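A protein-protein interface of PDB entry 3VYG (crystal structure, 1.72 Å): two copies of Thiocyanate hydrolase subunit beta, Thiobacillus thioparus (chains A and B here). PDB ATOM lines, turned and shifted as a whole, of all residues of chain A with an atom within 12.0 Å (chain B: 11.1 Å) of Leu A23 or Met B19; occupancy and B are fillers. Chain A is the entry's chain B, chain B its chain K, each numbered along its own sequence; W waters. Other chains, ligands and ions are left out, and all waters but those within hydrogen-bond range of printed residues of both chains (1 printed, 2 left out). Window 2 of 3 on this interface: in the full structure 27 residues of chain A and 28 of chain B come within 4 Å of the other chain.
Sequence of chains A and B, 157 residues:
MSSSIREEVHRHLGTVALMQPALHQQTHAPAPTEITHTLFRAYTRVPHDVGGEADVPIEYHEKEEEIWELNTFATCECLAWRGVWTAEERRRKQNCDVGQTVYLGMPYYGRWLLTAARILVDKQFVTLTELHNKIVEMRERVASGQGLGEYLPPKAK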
ATOM      1  N   ALA A  17     -15.941 -28.513   7.543  1.00  0.00           N
ATOM      2  CA  ALA A  17     -17.376 -28.242   7.404  1.00  0.00           C
ATOM      3  C   ALA A  17     -17.751 -26.857   7.889  1.00  0.00           C
ATOM      4  O   ALA A  17     -18.760 -26.336   7.411  1.00  0.00           O
ATOM      5  CB  ALA A  17     -18.184 -29.253   8.119  1.00  0.00           C
ATOM      6  N   LEU A  18     -16.948 -26.273   8.774  1.00  0.00           N
ATOM      7  CA  LEU A  18     -17.204 -24.856   9.233  1.00  0.00           C
ATOM      8  C   LEU A  18     -16.895 -23.872   8.119  1.00  0.00           C
ATOM      9  O   LEU A  18     -17.351 -22.750   8.150  1.00  0.00           O
ATOM     10  CB  LEU A  18     -16.263 -24.582  10.416  1.00  0.00           C
ATOM     11  CG  LEU A  18     -16.430 -25.505  11.575  1.00  0.00           C
ATOM     12  CD1 LEU A  18     -15.466 -25.015  12.575  1.00  0.00           C
ATOM     13  CD2 LEU A  18     -17.940 -25.444  12.093  1.00  0.00           C
ATOM     14  N   MET A  19     -16.101 -24.312   7.095  1.00  0.00           N
ATOM     15  CA  MET A  19     -15.564 -23.378   6.072  1.00  0.00           C
ATOM     16  C   MET A  19     -16.265 -23.587   4.765  1.00  0.00           C
ATOM     17  O   MET A  19     -15.872 -23.100   3.715  1.00  0.00           O
ATOM     18  CB  MET A  19     -14.053 -23.669   5.850  1.00  0.00           C
ATOM     19  CG  MET A  19     -13.267 -23.557   7.073  1.00  0.00           C
ATOM     20  SD  MET A  19     -11.565 -24.066   6.638  1.00  0.00           S
ATOM     21  CE  MET A  19     -10.889 -23.595   8.270  1.00  0.00           C
ATOM     22  N   GLN A  20     -17.342 -24.378   4.757  1.00  0.00           N
ATOM     23  CA  GLN A  20     -18.115 -24.602   3.472  1.00  0.00           C
ATOM     24  C   GLN A  20     -18.650 -23.287   2.969  1.00  0.00           C
ATOM     25  O   GLN A  20     -19.388 -22.578   3.727  1.00  0.00           O
ATOM     26  CB  GLN A  20     -19.235 -25.572   3.788  1.00  0.00           C
ATOM     27  CG  GLN A  20     -20.498 -25.647   2.882  1.00  0.00           C
ATOM     28  CD  GLN A  20     -20.292 -26.243   1.500  1.00  0.00           C
ATOM     29  OE1 GLN A  20     -19.996 -27.484   1.335  1.00  0.00           O
ATOM     30  NE2 GLN A  20     -20.617 -25.405   0.452  1.00  0.00           N
ATOM     31  N   PRO A  21     -18.402 -22.920   1.709  1.00  0.00           N
ATOM     32  CA  PRO A  21     -18.947 -21.722   1.125  1.00  0.00           C
ATOM     33  C   PRO A  21     -20.459 -21.578   1.100  1.00  0.00           C
ATOM     34  O   PRO A  21     -21.193 -22.555   0.945  1.00  0.00           O
ATOM     35  CB  PRO A  21     -18.330 -21.682  -0.308  1.00  0.00           C
ATOM     36  CG  PRO A  21     -17.244 -22.701  -0.220  1.00  0.00           C
ATOM     37  CD  PRO A  21     -17.640 -23.720   0.735  1.00  0.00           C
ATOM     38  N   ALA A  22     -20.917 -20.334   1.283  1.00  0.00           N
ATOM     39  CA  ALA A  22     -22.344 -20.108   1.344  1.00  0.00           C
ATOM     40  C   ALA A  22     -22.634 -18.692   0.936  1.00  0.00           C
ATOM     41  O   ALA A  22     -21.689 -17.850   0.926  1.00  0.00           O
ATOM     42  CB  ALA A  22     -22.811 -20.309   2.772  1.00  0.00           C
ATOM     43  N   LEU A  23     -23.893 -18.425   0.588  1.00  0.00           N
ATOM     44  CA  LEU A  23     -24.304 -17.059   0.373  1.00  0.00           C
ATOM     45  C   LEU A  23     -25.093 -16.774   1.660  1.00  0.00           C
ATOM     46  O   LEU A  23     -26.082 -17.391   1.978  1.00  0.00           O
ATOM     47  CB  LEU A  23     -25.122 -16.939  -0.953  1.00  0.00           C
ATOM     48  CG  LEU A  23     -24.349 -17.277  -2.229  1.00  0.00           C
ATOM     49  CD1 LEU A  23     -25.411 -16.997  -3.390  1.00  0.00           C
ATOM     50  CD2 LEU A  23     -23.057 -16.463  -2.424  1.00  0.00           C
ATOM     51  N   HIS A  24     -24.528 -15.832   2.441  1.00  0.00           N
ATOM     52  CA  HIS A  24     -25.039 -15.575   3.804  1.00  0.00           C
ATOM     53  C   HIS A  24     -25.585 -14.160   3.878  1.00  0.00           C
ATOM     54  O   HIS A  24     -24.816 -13.221   3.819  1.00  0.00           O
ATOM     55  CB  HIS A  24     -23.867 -15.726   4.764  1.00  0.00           C
ATOM     56  CG  HIS A  24     -24.244 -15.537   6.200  1.00  0.00           C
ATOM     57  ND1 HIS A  24     -24.642 -16.602   6.993  1.00  0.00           N
ATOM     58  CD2 HIS A  24     -24.223 -14.438   7.008  1.00  0.00           C
ATOM     59  CE1 HIS A  24     -24.890 -16.161   8.225  1.00  0.00           C
ATOM     60  NE2 HIS A  24     -24.594 -14.857   8.270  1.00  0.00           N
ATOM     61  N   GLN A  25     -26.897 -14.071   3.960  1.00  0.00           N
ATOM     62  CA  GLN A  25     -27.643 -12.804   4.038  1.00  0.00           C
ATOM     63  C   GLN A  25     -28.131 -12.503   5.475  1.00  0.00           C
ATOM     64  O   GLN A  25     -29.112 -13.059   5.951  1.00  0.00           O
ATOM     65  CB  GLN A  25     -28.851 -12.837   3.079  1.00  0.00           C
ATOM     66  CG  GLN A  25     -29.674 -11.543   3.134  1.00  0.00           C
ATOM     67  CD  GLN A  25     -28.890 -10.381   2.677  1.00  0.00           C
ATOM     68  OE1 GLN A  25     -28.629 -10.206   1.458  1.00  0.00           O
ATOM     69  NE2 GLN A  25     -28.538  -9.508   3.627  1.00  0.00           N
ATOM     70  N   GLN A  26     -27.443 -11.597   6.157  1.00  0.00           N
ATOM     71  CA  GLN A  26     -27.994 -11.222   7.474  1.00  0.00           C
ATOM     72  C   GLN A  26     -29.374 -10.577   7.346  1.00  0.00           C
ATOM     73  O   GLN A  26     -29.649  -9.824   6.395  1.00  0.00           O
ATOM     74  CB  GLN A  26     -27.041 -10.223   8.139  1.00  0.00           C
ATOM     75  CG  GLN A  26     -25.838 -10.908   8.803  1.00  0.00           C
ATOM     76  CD  GLN A  26     -24.899  -9.900   9.361  1.00  0.00           C
ATOM     77  OE1 GLN A  26     -25.315  -8.849   9.827  1.00  0.00           O
ATOM     78  NE2 GLN A  26     -23.594 -10.216   9.331  1.00  0.00           N
ATOM     79  N   THR A  27     -30.246 -10.831   8.330  1.00  0.00           N
ATOM     80  CA  THR A  27     -31.583 -10.234   8.285  1.00  0.00           C
ATOM     81  C   THR A  27     -31.783  -9.130   9.340  1.00  0.00           C
ATOM     82  O   THR A  27     -31.530  -9.403  10.517  1.00  0.00           O
ATOM     83  CB  THR A  27     -32.656 -11.324   8.502  1.00  0.00           C
ATOM     84  OG1 THR A  27     -32.538 -11.827   9.807  1.00  0.00           O
ATOM     85  CG2 THR A  27     -32.234 -12.567   7.759  1.00  0.00           C
ATOM     86  N   TYR A  43     -41.211 -17.983   9.203  1.00  0.00           N
ATOM     87  CA  TYR A  43     -40.875 -17.340  10.485  1.00  0.00           C
ATOM     88  C   TYR A  43     -41.911 -17.671  11.543  1.00  0.00           C
ATOM     89  O   TYR A  43     -41.544 -17.695  12.759  1.00  0.00           O
ATOM     90  CB  TYR A  43     -40.834 -15.810  10.313  1.00  0.00           C
ATOM     91  CG  TYR A  43     -39.519 -15.382   9.721  1.00  0.00           C
ATOM     92  CD1 TYR A  43     -39.473 -14.739   8.490  1.00  0.00           C
ATOM     93  CD2 TYR A  43     -38.305 -15.594  10.387  1.00  0.00           C
ATOM     94  CE1 TYR A  43     -38.265 -14.347   7.911  1.00  0.00           C
ATOM     95  CE2 TYR A  43     -37.104 -15.183   9.857  1.00  0.00           C
ATOM     96  CZ  TYR A  43     -37.082 -14.598   8.581  1.00  0.00           C
ATOM     97  OH  TYR A  43     -35.882 -14.194   8.040  1.00  0.00           O
ATOM     98  N   ARG B  11     -23.977  -3.196  -7.449  1.00  0.00           N
ATOM     99  CA  ARG B  11     -24.530  -4.539  -7.274  1.00  0.00           C
ATOM    100  C   ARG B  11     -23.387  -5.500  -6.859  1.00  0.00           C
ATOM    101  O   ARG B  11     -23.558  -6.423  -6.040  1.00  0.00           O
ATOM    102  CB  ARG B  11     -25.156  -5.056  -8.577  1.00  0.00           C
ATOM    103  CG  ARG B  11     -25.986  -6.347  -8.450  1.00  0.00           C
ATOM    104  CD  ARG B  11     -26.666  -6.664  -9.819  1.00  0.00           C
ATOM    105  NE  ARG B  11     -27.217  -5.417 -10.394  1.00  0.00           N
ATOM    106  CZ  ARG B  11     -26.792  -4.812 -11.507  1.00  0.00           C
ATOM    107  NH1 ARG B  11     -25.806  -5.325 -12.232  1.00  0.00           N
ATOM    108  NH2 ARG B  11     -27.361  -3.674 -11.903  1.00  0.00           N
ATOM    109  N   HIS B  12     -22.227  -5.309  -7.450  1.00  0.00           N
ATOM    110  CA  HIS B  12     -21.074  -6.174  -7.109  1.00  0.00           C
ATOM    111  C   HIS B  12     -20.696  -6.054  -5.633  1.00  0.00           C
ATOM    112  O   HIS B  12     -20.458  -7.050  -4.919  1.00  0.00           O
ATOM    113  CB  HIS B  12     -19.858  -5.797  -7.965  1.00  0.00           C
ATOM    114  CG  HIS B  12     -18.660  -6.698  -7.762  1.00  0.00           C
ATOM    115  ND1 HIS B  12     -17.558  -6.328  -7.011  1.00  0.00           N
ATOM    116  CD2 HIS B  12     -18.371  -7.930  -8.282  1.00  0.00           C
ATOM    117  CE1 HIS B  12     -16.634  -7.288  -7.072  1.00  0.00           C
ATOM    118  NE2 HIS B  12     -17.084  -8.242  -7.879  1.00  0.00           N
ATOM    119  N   LEU B  13     -20.598  -4.816  -5.183  1.00  0.00           N
ATOM    120  CA  LEU B  13     -20.156  -4.598  -3.823  1.00  0.00           C
ATOM    121  C   LEU B  13     -21.179  -5.288  -2.857  1.00  0.00           C
ATOM    122  O   LEU B  13     -20.797  -5.866  -1.799  1.00  0.00           O
ATOM    123  CB  LEU B  13     -19.992  -3.097  -3.575  1.00  0.00           C
ATOM    124  CG  LEU B  13     -18.725  -2.441  -4.162  1.00  0.00           C
ATOM    125  CD1 LEU B  13     -18.733  -0.890  -3.956  1.00  0.00           C
ATOM    126  CD2 LEU B  13     -17.422  -2.965  -3.512  1.00  0.00           C
ATOM    127  N   GLY B  14     -22.469  -5.225  -3.196  1.00  0.00           N
ATOM    128  CA  GLY B  14     -23.537  -5.900  -2.387  1.00  0.00           C
ATOM    129  C   GLY B  14     -23.364  -7.423  -2.389  1.00  0.00           C
ATOM    130  O   GLY B  14     -23.453  -8.069  -1.342  1.00  0.00           O
ATOM    131  N   THR B  15     -23.079  -7.971  -3.565  1.00  0.00           N
ATOM    132  CA  THR B  15     -22.914  -9.440  -3.724  1.00  0.00           C
ATOM    133  C   THR B  15     -21.689 -10.010  -2.994  1.00  0.00           C
ATOM    134  O   THR B  15     -21.800 -11.069  -2.317  1.00  0.00           O
ATOM    135  CB  THR B  15     -22.874  -9.807  -5.231  1.00  0.00           C
ATOM    136  OG1 THR B  15     -24.026  -9.238  -5.857  1.00  0.00           O
ATOM    137  CG2 THR B  15     -22.869 -11.329  -5.474  1.00  0.00           C
ATOM    138  N   VAL B  16     -20.533  -9.340  -3.111  1.00  0.00           N
ATOM    139  CA  VAL B  16     -19.296  -9.698  -2.377  1.00  0.00           C
ATOM    140  C   VAL B  16     -19.566 -10.045  -0.890  1.00  0.00           C
ATOM    141  O   VAL B  16     -18.866 -10.938  -0.310  1.00  0.00           O
ATOM    142  CB  VAL B  16     -18.182  -8.447  -2.433  1.00  0.00           C
ATOM    143  N   ALA B  17     -20.474  -9.273  -0.299  1.00  0.00           N
ATOM    144  CA  ALA B  17     -20.664  -9.337   1.140  1.00  0.00           C
ATOM    145  C   ALA B  17     -21.246 -10.700   1.587  1.00  0.00           C
ATOM    146  O   ALA B  17     -20.960 -11.178   2.710  1.00  0.00           O
ATOM    147  CB  ALA B  17     -21.550  -8.285   1.557  1.00  0.00           C
ATOM    148  N   LEU B  18     -22.038 -11.273   0.695  1.00  0.00           N
ATOM    149  CA  LEU B  18     -22.664 -12.570   0.897  1.00  0.00           C
ATOM    150  C   LEU B  18     -21.647 -13.660   0.855  1.00  0.00           C
ATOM    151  O   LEU B  18     -21.898 -14.712   1.458  1.00  0.00           O
ATOM    152  CB  LEU B  18     -23.719 -12.841  -0.175  1.00  0.00           C
ATOM    153  CG  LEU B  18     -24.875 -11.903  -0.415  1.00  0.00           C
ATOM    154  CD1 LEU B  18     -25.515 -12.527  -1.745  1.00  0.00           C
ATOM    155  CD2 LEU B  18     -25.830 -11.809   0.803  1.00  0.00           C
ATOM    156  N   MET B  19     -20.462 -13.417   0.275  1.00  0.00           N
ATOM    157  CA  MET B  19     -19.404 -14.450   0.250  1.00  0.00           C
ATOM    158  C   MET B  19     -18.366 -14.250   1.271  1.00  0.00           C
ATOM    159  O   MET B  19     -17.373 -14.932   1.278  1.00  0.00           O
ATOM    160  CB  MET B  19     -18.751 -14.341  -1.164  1.00  0.00           C
ATOM    161  CG  MET B  19     -19.762 -14.526  -2.154  1.00  0.00           C
ATOM    162  SD  MET B  19     -18.999 -14.265  -3.852  1.00  0.00           S
ATOM    163  CE  MET B  19     -20.387 -14.857  -4.805  1.00  0.00           C
ATOM    164  N   GLN B  20     -18.618 -13.335   2.242  1.00  0.00           N
ATOM    165  CA  GLN B  20     -17.637 -13.123   3.267  1.00  0.00           C
ATOM    166  C   GLN B  20     -17.384 -14.447   3.950  1.00  0.00           C
ATOM    167  O   GLN B  20     -18.310 -14.976   4.590  1.00  0.00           O
ATOM    168  CB  GLN B  20     -18.203 -12.092   4.234  1.00  0.00           C
ATOM    169  CG  GLN B  20     -17.509 -12.005   5.619  1.00  0.00           C
ATOM    170  CD  GLN B  20     -16.079 -11.548   5.539  1.00  0.00           C
ATOM    171  OE1 GLN B  20     -15.768 -10.475   4.956  1.00  0.00           O
ATOM    172  NE2 GLN B  20     -15.189 -12.363   6.119  1.00  0.00           N
ATOM    173  N   PRO B  21     -16.127 -14.942   3.927  1.00  0.00           N
ATOM    174  CA  PRO B  21     -15.784 -16.175   4.642  1.00  0.00           C
ATOM    175  C   PRO B  21     -16.128 -16.106   6.094  1.00  0.00           C
ATOM    176  O   PRO B  21     -16.025 -15.023   6.738  1.00  0.00           O
ATOM    177  CB  PRO B  21     -14.249 -16.265   4.507  1.00  0.00           C
ATOM    178  CG  PRO B  21     -14.001 -15.660   3.187  1.00  0.00           C
ATOM    179  CD  PRO B  21     -14.937 -14.425   3.199  1.00  0.00           C
ATOM    180  N   ALA B  22     -16.442 -17.258   6.649  1.00  0.00           N
ATOM    181  CA  ALA B  22     -16.728 -17.386   8.045  1.00  0.00           C
ATOM    182  C   ALA B  22     -16.523 -18.789   8.508  1.00  0.00           C
ATOM    183  O   ALA B  22     -16.395 -19.733   7.642  1.00  0.00           O
ATOM    184  CB  ALA B  22     -18.290 -16.996   8.245  1.00  0.00           C
ATOM    185  N   LEU B  23     -16.396 -18.968   9.833  1.00  0.00           N
ATOM    186  CA  LEU B  23     -16.380 -20.283  10.445  1.00  0.00           C
ATOM    187  C   LEU B  23     -17.864 -20.386  10.886  1.00  0.00           C
ATOM    188  O   LEU B  23     -18.278 -19.667  11.819  1.00  0.00           O
ATOM    189  CB  LEU B  23     -15.421 -20.284  11.680  1.00  0.00           C
ATOM    190  CG  LEU B  23     -13.953 -20.249  11.153  1.00  0.00           C
ATOM    191  CD1 LEU B  23     -13.025 -20.047  12.272  1.00  0.00           C
ATOM    192  CD2 LEU B  23     -13.514 -21.522  10.421  1.00  0.00           C
ATOM    193  N   HIS B  24     -18.624 -21.259  10.223  1.00  0.00           N
ATOM    194  CA  HIS B  24     -20.065 -21.306  10.432  1.00  0.00           C
ATOM    195  C   HIS B  24     -20.391 -22.598  11.089  1.00  0.00           C
ATOM    196  O   HIS B  24     -20.265 -23.634  10.477  1.00  0.00           O
ATOM    197  CB  HIS B  24     -20.738 -21.213   9.057  1.00  0.00           C
ATOM    198  CG  HIS B  24     -22.241 -21.223   9.106  1.00  0.00           C
ATOM    199  ND1 HIS B  24     -22.976 -20.074   9.318  1.00  0.00           N
ATOM    200  CD2 HIS B  24     -23.130 -22.230   8.916  1.00  0.00           C
ATOM    201  CE1 HIS B  24     -24.268 -20.371   9.265  1.00  0.00           C
ATOM    202  NE2 HIS B  24     -24.387 -21.685   9.098  1.00  0.00           N
HETATM  203  O   HOH W   1     -22.057 -12.474   4.692  1.00  0.00           O
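The backbone NH (N) of His B24 lies within hydrogen-bond range of the backbone carbonyl oxygen (O) of Leu A18, at 2.9 Å. O of Leu B18 lies within hydrogen-bond range of N of His A24, 3.0 Å away. O of Ala B22 sits close to O of Leu A18. The backbone carbonyl oxygen (O) of Leu B18 lies close to the backbone carbonyl oxygen (O) of Ala A22 (3.2 Å).
Among the printed residues, pairs that only touch across the chains: Leu A18 with Leu B23 (3.5 Å), Met A19 with Leu B23 (3.9 Å), Leu A23 with Leu B18 (3.5 Å), Leu A23 with Met B19 (3.8 Å) and Gln A25 with Leu B18 (3.3 Å).
Leu A23 touches two residues of chain B. Ala A22 touches one residue of chain B. Of chain B, only Leu B18 (3.0 Å) comes within 4 Å of His A24. No residue of chain A comes within 4 Å of Ala B17. Pro B21 touches none of the printed residues of chain A. Of the printed residues of chain A, His B24 touches Leu A18 (2.9 Å). Printed residues of chain B within 4 Å of Met A19: Leu B23. Of the printed residues of chain B, Leu A18 touches Ala B22 (3.2 Å), Leu B23 (3.5 Å) and His B24 (2.9 Å). Printed residues of chain B within 4 Å of Gln A25: Leu B18 (3.3 Å). Of the printed residues of chain A, Leu B23 touches Leu A18 and Met A19. The nearest residue of chain B that does not touch Leu A23 is Thr B15 (5.5 Å). The nearest residue of chain A that does not touch Met B19 is Ala A22 (4.2 Å).
Of the 14 printed residues of chain B, 5 touch a printed residue of chain A. Of the 12 printed residues of chain A, 6 touch a printed residue of chain B. Printed residues of chain A that touch a printed residue of chain B: Leu A18, Met A19, Ala A22, Leu A23, His A24 and Gln A25. Hydrophobic or aromatic side chains of chain A that line the printed part of chain B: Leu A18, Met A19, Leu A23 and His A24. Among the printed residues, 9 pairs touch across the chains.
Leu A18 touches Ala B22, and with the chains exchanged Ala A22 touches Leu B18. Leu A18 touches Leu B23, and with the chains exchanged Leu A23 touches Leu B18. Leu A18 touches His B24, and with the chains exchanged His A24 touches Leu B18. Met A19 touches Leu B23, and with the chains exchanged Leu A23 touches Met B19. Positions printed for both chains: 17, 18, 19, 20, 21, 22, 23 and 24. Of the 9 pairs that touch across the chains among the printed residues, 8 have their exchanged pair printed and touching as well.
Water W1 lies within hydrogen-bond range of O of Ala B17 and O of His A24.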
